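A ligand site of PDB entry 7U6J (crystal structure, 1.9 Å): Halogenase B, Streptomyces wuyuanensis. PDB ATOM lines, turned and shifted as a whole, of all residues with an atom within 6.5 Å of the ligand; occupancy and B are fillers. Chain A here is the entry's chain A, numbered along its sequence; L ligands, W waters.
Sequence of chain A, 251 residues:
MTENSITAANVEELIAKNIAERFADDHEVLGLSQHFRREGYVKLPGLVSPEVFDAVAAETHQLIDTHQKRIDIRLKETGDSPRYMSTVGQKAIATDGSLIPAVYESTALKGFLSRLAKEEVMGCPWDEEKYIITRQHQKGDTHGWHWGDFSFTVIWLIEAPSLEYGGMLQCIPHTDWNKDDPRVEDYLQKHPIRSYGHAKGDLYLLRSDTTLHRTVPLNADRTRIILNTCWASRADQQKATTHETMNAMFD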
ATOM      1  N   LEU A  75     -20.164  11.572 -10.180  1.00  0.00           N
ATOM      2  CA  LEU A  75     -21.584  11.511  -9.851  1.00  0.00           C
ATOM      3  C   LEU A  75     -22.303  10.574 -10.807  1.00  0.00           C
ATOM      4  O   LEU A  75     -22.355  10.838 -12.014  1.00  0.00           O
ATOM      5  CB  LEU A  75     -22.227  12.905  -9.885  1.00  0.00           C
ATOM      6  CG  LEU A  75     -21.700  13.887  -8.843  1.00  0.00           C
ATOM      7  CD1 LEU A  75     -22.147  15.333  -9.102  1.00  0.00           C
ATOM      8  CD2 LEU A  75     -22.120  13.425  -7.463  1.00  0.00           C
ATOM      9  N   THR A  78     -24.935  11.896 -13.415  1.00  0.00           N
ATOM     10  CA  THR A  78     -24.480  12.476 -14.676  1.00  0.00           C
ATOM     11  C   THR A  78     -23.449  11.571 -15.358  1.00  0.00           C
ATOM     12  O   THR A  78     -22.484  12.035 -15.962  1.00  0.00           O
ATOM     13  CB  THR A  78     -23.912  13.882 -14.480  1.00  0.00           C
ATOM     14  OG1 THR A  78     -22.796  13.840 -13.587  1.00  0.00           O
ATOM     15  CG2 THR A  78     -24.975  14.821 -13.916  1.00  0.00           C
ATOM     16  N   SER A  81     -19.519  11.547 -14.336  1.00  0.00           N
ATOM     17  CA  SER A  81     -18.622  12.616 -14.721  1.00  0.00           C
ATOM     18  C   SER A  81     -17.996  13.242 -13.472  1.00  0.00           C
ATOM     19  O   SER A  81     -18.574  13.198 -12.384  1.00  0.00           O
ATOM     20  CB  SER A  81     -19.372  13.668 -15.550  1.00  0.00           C
ATOM     21  OG  SER A  81     -20.464  14.207 -14.838  1.00  0.00           O
ATOM     22  N   ARG A  83     -16.375  15.932 -10.659  1.00  0.00           N
ATOM     23  CA  ARG A  83     -16.333  17.273 -10.085  1.00  0.00           C
ATOM     24  C   ARG A  83     -15.019  17.325  -9.298  1.00  0.00           C
ATOM     25  O   ARG A  83     -14.938  16.823  -8.177  1.00  0.00           O
ATOM     26  CB  ARG A  83     -17.531  17.552  -9.173  1.00  0.00           C
ATOM     27  CG  ARG A  83     -18.889  17.209  -9.787  1.00  0.00           C
ATOM     28  CD  ARG A  83     -19.271  18.134 -10.957  1.00  0.00           C
ATOM     29  NE  ARG A  83     -20.612  17.803 -11.417  1.00  0.00           N
ATOM     30  CZ  ARG A  83     -20.889  16.754 -12.172  1.00  0.00           C
ATOM     31  NH1 ARG A  83     -19.919  15.993 -12.678  1.00  0.00           N
ATOM     32  NH2 ARG A  83     -22.156  16.426 -12.398  1.00  0.00           N
ATOM     33  N   GLU A 129     -29.645  26.007  -3.643  1.00  0.00           N
ATOM     34  CA  GLU A 129     -29.124  26.156  -5.001  1.00  0.00           C
ATOM     35  C   GLU A 129     -29.081  27.613  -5.468  1.00  0.00           C
ATOM     36  O   GLU A 129     -28.626  27.863  -6.594  1.00  0.00           O
ATOM     37  CB  GLU A 129     -29.939  25.323  -5.982  1.00  0.00           C
ATOM     38  CG  GLU A 129     -29.251  25.155  -7.371  1.00  0.00           C
ATOM     39  CD  GLU A 129     -29.422  23.764  -7.968  1.00  0.00           C
ATOM     40  OE1 GLU A 129     -30.114  22.940  -7.338  1.00  0.00           O
ATOM     41  OE2 GLU A 129     -28.865  23.520  -9.067  1.00  0.00           O
ATOM     42  N   ILE A 132     -23.841  29.509  -5.534  1.00  0.00           N
ATOM     43  CA  ILE A 132     -22.697  28.724  -5.066  1.00  0.00           C
ATOM     44  C   ILE A 132     -21.452  29.277  -5.737  1.00  0.00           C
ATOM     45  O   ILE A 132     -21.525  30.051  -6.693  1.00  0.00           O
ATOM     46  CB  ILE A 132     -22.861  27.197  -5.346  1.00  0.00           C
ATOM     47  CG1 ILE A 132     -23.173  26.916  -6.822  1.00  0.00           C
ATOM     48  CG2 ILE A 132     -23.969  26.588  -4.449  1.00  0.00           C
ATOM     49  CD1 ILE A 132     -21.922  26.706  -7.708  1.00  0.00           C
ATOM     50  N   HIS A 143     -15.514  21.016 -14.066  1.00  0.00           N
ATOM     51  CA  HIS A 143     -16.916  20.767 -13.771  1.00  0.00           C
ATOM     52  C   HIS A 143     -17.441  19.875 -14.902  1.00  0.00           C
ATOM     53  O   HIS A 143     -17.780  20.368 -15.987  1.00  0.00           O
ATOM     54  CB  HIS A 143     -17.690  22.080 -13.637  1.00  0.00           C
ATOM     55  CG  HIS A 143     -18.980  21.935 -12.897  1.00  0.00           C
ATOM     56  ND1 HIS A 143     -19.527  22.965 -12.153  1.00  0.00           N
ATOM     57  CD2 HIS A 143     -19.839  20.895 -12.777  1.00  0.00           C
ATOM     58  CE1 HIS A 143     -20.654  22.561 -11.615  1.00  0.00           C
ATOM     59  NE2 HIS A 143     -20.870  21.308 -11.983  1.00  0.00           N
ATOM     60  N   GLY A 144     -17.469  18.573 -14.662  1.00  0.00           N
ATOM     61  CA  GLY A 144     -17.760  17.612 -15.709  1.00  0.00           C
ATOM     62  C   GLY A 144     -19.181  17.702 -16.240  1.00  0.00           C
ATOM     63  O   GLY A 144     -20.025  18.440 -15.730  1.00  0.00           O
ATOM     64  N   TRP A 145     -19.455  16.919 -17.290  1.00  0.00           N
ATOM     65  CA  TRP A 145     -20.744  16.970 -17.974  1.00  0.00           C
ATOM     66  C   TRP A 145     -21.902  16.846 -16.982  1.00  0.00           C
ATOM     67  O   TRP A 145     -21.891  15.981 -16.112  1.00  0.00           O
ATOM     68  CB  TRP A 145     -20.851  15.864 -19.020  1.00  0.00           C
ATOM     69  CG  TRP A 145     -20.026  16.090 -20.268  1.00  0.00           C
ATOM     70  CD1 TRP A 145     -18.957  15.340 -20.693  1.00  0.00           C
ATOM     71  CD2 TRP A 145     -20.235  17.084 -21.285  1.00  0.00           C
ATOM     72  NE1 TRP A 145     -18.477  15.825 -21.883  1.00  0.00           N
ATOM     73  CE2 TRP A 145     -19.243  16.901 -22.268  1.00  0.00           C
ATOM     74  CE3 TRP A 145     -21.171  18.115 -21.456  1.00  0.00           C
ATOM     75  CZ2 TRP A 145     -19.161  17.703 -23.413  1.00  0.00           C
ATOM     76  CZ3 TRP A 145     -21.079  18.921 -22.593  1.00  0.00           C
ATOM     77  CH2 TRP A 145     -20.086  18.708 -23.555  1.00  0.00           C
ATOM     78  N   HIS A 146     -22.893  17.723 -17.127  1.00  0.00           N
ATOM     79  CA  HIS A 146     -23.989  17.725 -16.184  1.00  0.00           C
ATOM     80  C   HIS A 146     -25.129  18.583 -16.726  1.00  0.00           C
ATOM     81  O   HIS A 146     -24.998  19.261 -17.754  1.00  0.00           O
ATOM     82  CB  HIS A 146     -23.538  18.234 -14.803  1.00  0.00           C
ATOM     83  CG  HIS A 146     -23.198  19.693 -14.771  1.00  0.00           C
ATOM     84  ND1 HIS A 146     -22.018  20.202 -15.274  1.00  0.00           N
ATOM     85  CD2 HIS A 146     -23.889  20.753 -14.292  1.00  0.00           C
ATOM     86  CE1 HIS A 146     -21.994  21.514 -15.113  1.00  0.00           C
ATOM     87  NE2 HIS A 146     -23.126  21.873 -14.517  1.00  0.00           N
ATOM     88  N   TRP A 147     -26.243  18.538 -16.024  1.00  0.00           N
ATOM     89  CA  TRP A 147     -27.338  19.469 -16.154  1.00  0.00           C
ATOM     90  C   TRP A 147     -27.582  20.087 -14.779  1.00  0.00           C
ATOM     91  O   TRP A 147     -27.080  19.582 -13.770  1.00  0.00           O
ATOM     92  CB  TRP A 147     -28.639  18.788 -16.632  1.00  0.00           C
ATOM     93  CG  TRP A 147     -28.641  18.171 -18.010  1.00  0.00           C
ATOM     94  CD1 TRP A 147     -29.141  18.724 -19.160  1.00  0.00           C
ATOM     95  CD2 TRP A 147     -28.183  16.862 -18.366  1.00  0.00           C
ATOM     96  NE1 TRP A 147     -29.000  17.847 -20.205  1.00  0.00           N
ATOM     97  CE2 TRP A 147     -28.414  16.694 -19.752  1.00  0.00           C
ATOM     98  CE3 TRP A 147     -27.583  15.809 -17.662  1.00  0.00           C
ATOM     99  CZ2 TRP A 147     -28.078  15.525 -20.436  1.00  0.00           C
ATOM    100  CZ3 TRP A 147     -27.252  14.656 -18.346  1.00  0.00           C
ATOM    101  CH2 TRP A 147     -27.495  14.521 -19.718  1.00  0.00           C
ATOM    102  N   GLY A 148     -28.342  21.164 -14.748  1.00  0.00           N
ATOM    103  CA  GLY A 148     -28.801  21.743 -13.509  1.00  0.00           C
ATOM    104  C   GLY A 148     -30.223  21.308 -13.228  1.00  0.00           C
ATOM    105  O   GLY A 148     -30.965  20.918 -14.132  1.00  0.00           O
ATOM    106  N   ASP A 149     -30.601  21.369 -11.952  1.00  0.00           N
ATOM    107  CA  ASP A 149     -31.974  21.068 -11.562  1.00  0.00           C
ATOM    108  C   ASP A 149     -32.936  22.201 -11.904  1.00  0.00           C
ATOM    109  O   ASP A 149     -34.154  21.964 -11.917  1.00  0.00           O
ATOM    110  CB  ASP A 149     -32.053  20.753 -10.063  1.00  0.00           C
ATOM    111  CG  ASP A 149     -31.505  19.379  -9.713  1.00  0.00           C
ATOM    112  OD1 ASP A 149     -32.113  18.377 -10.131  1.00  0.00           O
ATOM    113  OD2 ASP A 149     -30.450  19.308  -9.038  1.00  0.00           O
ATOM    114  N   PHE A 150     -32.442  23.411 -12.168  1.00  0.00           N
ATOM    115  CA  PHE A 150     -33.314  24.558 -12.409  1.00  0.00           C
ATOM    116  C   PHE A 150     -32.883  25.276 -13.689  1.00  0.00           C
ATOM    117  O   PHE A 150     -31.896  24.923 -14.330  1.00  0.00           O
ATOM    118  CB  PHE A 150     -33.322  25.491 -11.182  1.00  0.00           C
ATOM    119  CG  PHE A 150     -33.827  24.812  -9.941  1.00  0.00           C
ATOM    120  CD1 PHE A 150     -35.179  24.596  -9.759  1.00  0.00           C
ATOM    121  CD2 PHE A 150     -32.942  24.359  -8.961  1.00  0.00           C
ATOM    122  CE1 PHE A 150     -35.654  23.949  -8.619  1.00  0.00           C
ATOM    123  CE2 PHE A 150     -33.410  23.708  -7.827  1.00  0.00           C
ATOM    124  CZ  PHE A 150     -34.761  23.505  -7.652  1.00  0.00           C
ATOM    125  N   THR A 153     -29.402  29.902 -15.122  1.00  0.00           N
ATOM    126  CA  THR A 153     -28.134  30.056 -14.417  1.00  0.00           C
ATOM    127  C   THR A 153     -27.325  31.196 -15.035  1.00  0.00           C
ATOM    128  O   THR A 153     -27.115  31.230 -16.247  1.00  0.00           O
ATOM    129  CB  THR A 153     -27.339  28.743 -14.497  1.00  0.00           C
ATOM    130  OG1 THR A 153     -28.036  27.725 -13.762  1.00  0.00           O
ATOM    131  CG2 THR A 153     -25.969  28.902 -13.912  1.00  0.00           C
ATOM    132  N   TRP A 177     -32.371  15.936 -18.443  1.00  0.00           N
ATOM    133  CA  TRP A 177     -31.620  15.221 -17.418  1.00  0.00           C
ATOM    134  C   TRP A 177     -32.479  14.084 -16.887  1.00  0.00           C
ATOM    135  O   TRP A 177     -33.463  14.318 -16.166  1.00  0.00           O
ATOM    136  CB  TRP A 177     -31.218  16.173 -16.297  1.00  0.00           C
ATOM    137  CG  TRP A 177     -30.218  15.592 -15.319  1.00  0.00           C
ATOM    138  CD1 TRP A 177     -29.546  14.393 -15.428  1.00  0.00           C
ATOM    139  CD2 TRP A 177     -29.779  16.187 -14.087  1.00  0.00           C
ATOM    140  NE1 TRP A 177     -28.713  14.220 -14.350  1.00  0.00           N
ATOM    141  CE2 TRP A 177     -28.834  15.296 -13.507  1.00  0.00           C
ATOM    142  CE3 TRP A 177     -30.075  17.381 -13.424  1.00  0.00           C
ATOM    143  CZ2 TRP A 177     -28.200  15.576 -12.295  1.00  0.00           C
ATOM    144  CZ3 TRP A 177     -29.434  17.656 -12.218  1.00  0.00           C
ATOM    145  CH2 TRP A 177     -28.508  16.759 -11.670  1.00  0.00           C
ATOM    146  N   SER A 208     -29.906  25.891 -17.800  1.00  0.00           N
ATOM    147  CA  SER A 208     -29.137  24.804 -17.214  1.00  0.00           C
ATOM    148  C   SER A 208     -29.905  23.484 -17.150  1.00  0.00           C
ATOM    149  O   SER A 208     -29.278  22.416 -17.073  1.00  0.00           O
ATOM    150  CB  SER A 208     -28.654  25.207 -15.812  1.00  0.00           C
ATOM    151  OG  SER A 208     -29.597  26.049 -15.154  1.00  0.00           O
ATOM    152  N   ASN A 228     -22.048  31.155  -9.282  1.00  0.00           N
ATOM    153  CA  ASN A 228     -23.229  30.648  -9.969  1.00  0.00           C
ATOM    154  C   ASN A 228     -24.456  31.171  -9.229  1.00  0.00           C
ATOM    155  O   ASN A 228     -24.756  30.702  -8.131  1.00  0.00           O
ATOM    156  CB  ASN A 228     -23.203  29.109 -10.011  1.00  0.00           C
ATOM    157  CG  ASN A 228     -24.441  28.501 -10.676  1.00  0.00           C
ATOM    158  OD1 ASN A 228     -25.538  29.040 -10.603  1.00  0.00           O
ATOM    159  ND2 ASN A 228     -24.252  27.348 -11.304  1.00  0.00           N
ATOM    160  N   CYS A 230     -28.378  31.076  -9.531  1.00  0.00           N
ATOM    161  CA  CYS A 230     -29.295  30.189 -10.251  1.00  0.00           C
ATOM    162  C   CYS A 230     -30.732  30.549  -9.912  1.00  0.00           C
ATOM    163  O   CYS A 230     -31.142  30.463  -8.748  1.00  0.00           O
ATOM    164  CB  CYS A 230     -29.015  28.730  -9.905  1.00  0.00           C
ATOM    165  SG  CYS A 230     -30.064  27.564 -10.789  1.00  0.00           S
ATOM    166  N   THR A 245     -26.794  15.675  -6.373  1.00  0.00           N
ATOM    167  CA  THR A 245     -25.540  16.242  -6.869  1.00  0.00           C
ATOM    168  C   THR A 245     -25.157  17.484  -6.080  1.00  0.00           C
ATOM    169  O   THR A 245     -23.979  17.720  -5.808  1.00  0.00           O
ATOM    170  CB  THR A 245     -25.613  16.560  -8.370  1.00  0.00           C
ATOM    171  OG1 THR A 245     -26.488  17.670  -8.607  1.00  0.00           O
ATOM    172  CG2 THR A 245     -26.074  15.332  -9.185  1.00  0.00           C
ATOM    173  N   MET A 246     -26.163  18.253  -5.680  1.00  0.00           N
ATOM    174  CA  MET A 246     -25.956  19.449  -4.871  1.00  0.00           C
ATOM    175  C   MET A 246     -25.448  19.066  -3.476  1.00  0.00           C
ATOM    176  O   MET A 246     -24.498  19.680  -2.957  1.00  0.00           O
ATOM    177  CB  MET A 246     -27.285  20.191  -4.775  1.00  0.00           C
ATOM    178  CG  MET A 246     -27.541  21.267  -5.832  1.00  0.00           C
ATOM    179  SD  MET A 246     -26.268  22.411  -6.347  1.00  0.00           S
ATOM    180  CE  MET A 246     -26.176  23.470  -4.890  1.00  0.00           C
ATOM    181  N   MET A 249     -21.698  17.999  -3.681  1.00  0.00           N
ATOM    182  CA  MET A 249     -20.611  18.937  -3.941  1.00  0.00           C
ATOM    183  C   MET A 249     -20.472  20.107  -2.966  1.00  0.00           C
ATOM    184  O   MET A 249     -19.414  20.754  -2.973  1.00  0.00           O
ATOM    185  CB  MET A 249     -20.658  19.552  -5.353  1.00  0.00           C
ATOM    186  CG  MET A 249     -20.651  18.606  -6.574  1.00  0.00           C
ATOM    187  SD  MET A 249     -21.615  19.217  -7.960  1.00  0.00           S
ATOM    188  CE  MET A 249     -20.493  20.485  -8.507  1.00  0.00           C
ATOM    189  N   PHE A 250     -21.479  20.418  -2.144  1.00  0.00           N
ATOM    190  CA  PHE A 250     -21.388  21.610  -1.297  1.00  0.00           C
ATOM    191  C   PHE A 250     -21.758  21.265   0.140  1.00  0.00           C
ATOM    192  O   PHE A 250     -22.608  20.426   0.393  1.00  0.00           O
ATOM    193  CB  PHE A 250     -22.295  22.730  -1.810  1.00  0.00           C
ATOM    194  CG  PHE A 250     -22.067  23.082  -3.241  1.00  0.00           C
ATOM    195  CD1 PHE A 250     -21.095  24.011  -3.599  1.00  0.00           C
ATOM    196  CD2 PHE A 250     -22.793  22.468  -4.254  1.00  0.00           C
ATOM    197  CE1 PHE A 250     -20.873  24.337  -4.924  1.00  0.00           C
ATOM    198  CE2 PHE A 250     -22.562  22.773  -5.572  1.00  0.00           C
ATOM    199  CZ  PHE A 250     -21.617  23.718  -5.905  1.00  0.00           C
HETATM  200  N1  LIG L   1     -26.339  19.613 -10.796  1.00  0.00           N
HETATM  201  C1  LIG L   1     -25.020  20.246 -10.791  1.00  0.00           C
HETATM  202  C2  LIG L   1     -23.953  19.218 -11.151  1.00  0.00           C
HETATM  203  O1  LIG L   1     -22.759  19.532 -11.181  1.00  0.00           O
HETATM  204  C3  LIG L   1     -24.721  20.866  -9.437  1.00  0.00           C
HETATM  205  C4  LIG L   1     -24.315  22.327  -9.494  1.00  0.00           C
HETATM  206  C5  LIG L   1     -25.472  23.192  -9.996  1.00  0.00           C
HETATM  207  C6  LIG L   1     -25.328  24.641  -9.544  1.00  0.00           C
HETATM  208  N2  LIG L   1     -26.624  25.381  -9.586  1.00  0.00           N
HETATM  209  O2  LIG L   1     -24.288  18.043 -11.362  1.00  0.00           O
HETATM  210  O   HOH W   1     -28.546  21.131  -9.885  1.00  0.00           O
HETATM  211  O   HOH W   2     -26.375  27.689  -7.913  1.00  0.00           O
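A ring nitrogen (NE2) of His 143 is in hydrogen-bond range of an oxygen (O1) of the ligand (2.7 Å).
The guanidinium group of Arg 83 is in salt-bridge range of an oxygen (O1) of the ligand (2.8 Å).
OG1 of Thr 245 is in hydrogen-bond range of N1 of the ligand (2.9 Å).
The side-chain carboxylate (OE2) of Glu 129 is in salt-bridge range of a nitrogen (N2) of the ligand.
O of Trp 147 lies within hydrogen-bond range of N1 of the ligand, 3.1 Å away.
A ring nitrogen (NE2) of His 143 sits close to a ring nitrogen (NE2) of His 146, 3.4 Å away.
NH2 of Arg 83 lies within hydrogen-bond range of OG1 of Thr 78, 2.9 Å away.
The side-chain hydroxyl (OG) of Ser 81 lies within hydrogen-bond range of the guanidinium group (NH1) of Arg 83, at 2.9 Å.
The backbone carbonyl oxygen (O) of Ile 132 is in hydrogen-bond range of the backbone NH (N) of Asn 228 (2.9 Å).
The backbone carbonyl oxygen (O) of Gly 144 is in hydrogen-bond range of a ring nitrogen (ND1) of His 146.
Water W1 lies within hydrogen-bond range of OE2 of Glu 129 (2.5 Å), OD2 of Asp 149 (2.8 Å) and N1 of the ligand (2.8 Å).
Water W2 lies within hydrogen-bond range of O of Glu 129 (2.6 Å), N2 of the ligand (2.9 Å) and OD1 of Asn 228 (3.1 Å).
The side-chain sulfur (SD) of Met 249 lies close to an oxygen (O1) of the ligand (3.4 Å).
Merely in contact with the ligand: His 146, Trp 177, Asn 228 and Met 246.
Ten residues have an atom within 4 Å of the ligand: Arg 83, Glu 129, His 143, His 146, Trp 147, Trp 177, Asn 228, Thr 245, Met 246 and Met 249.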
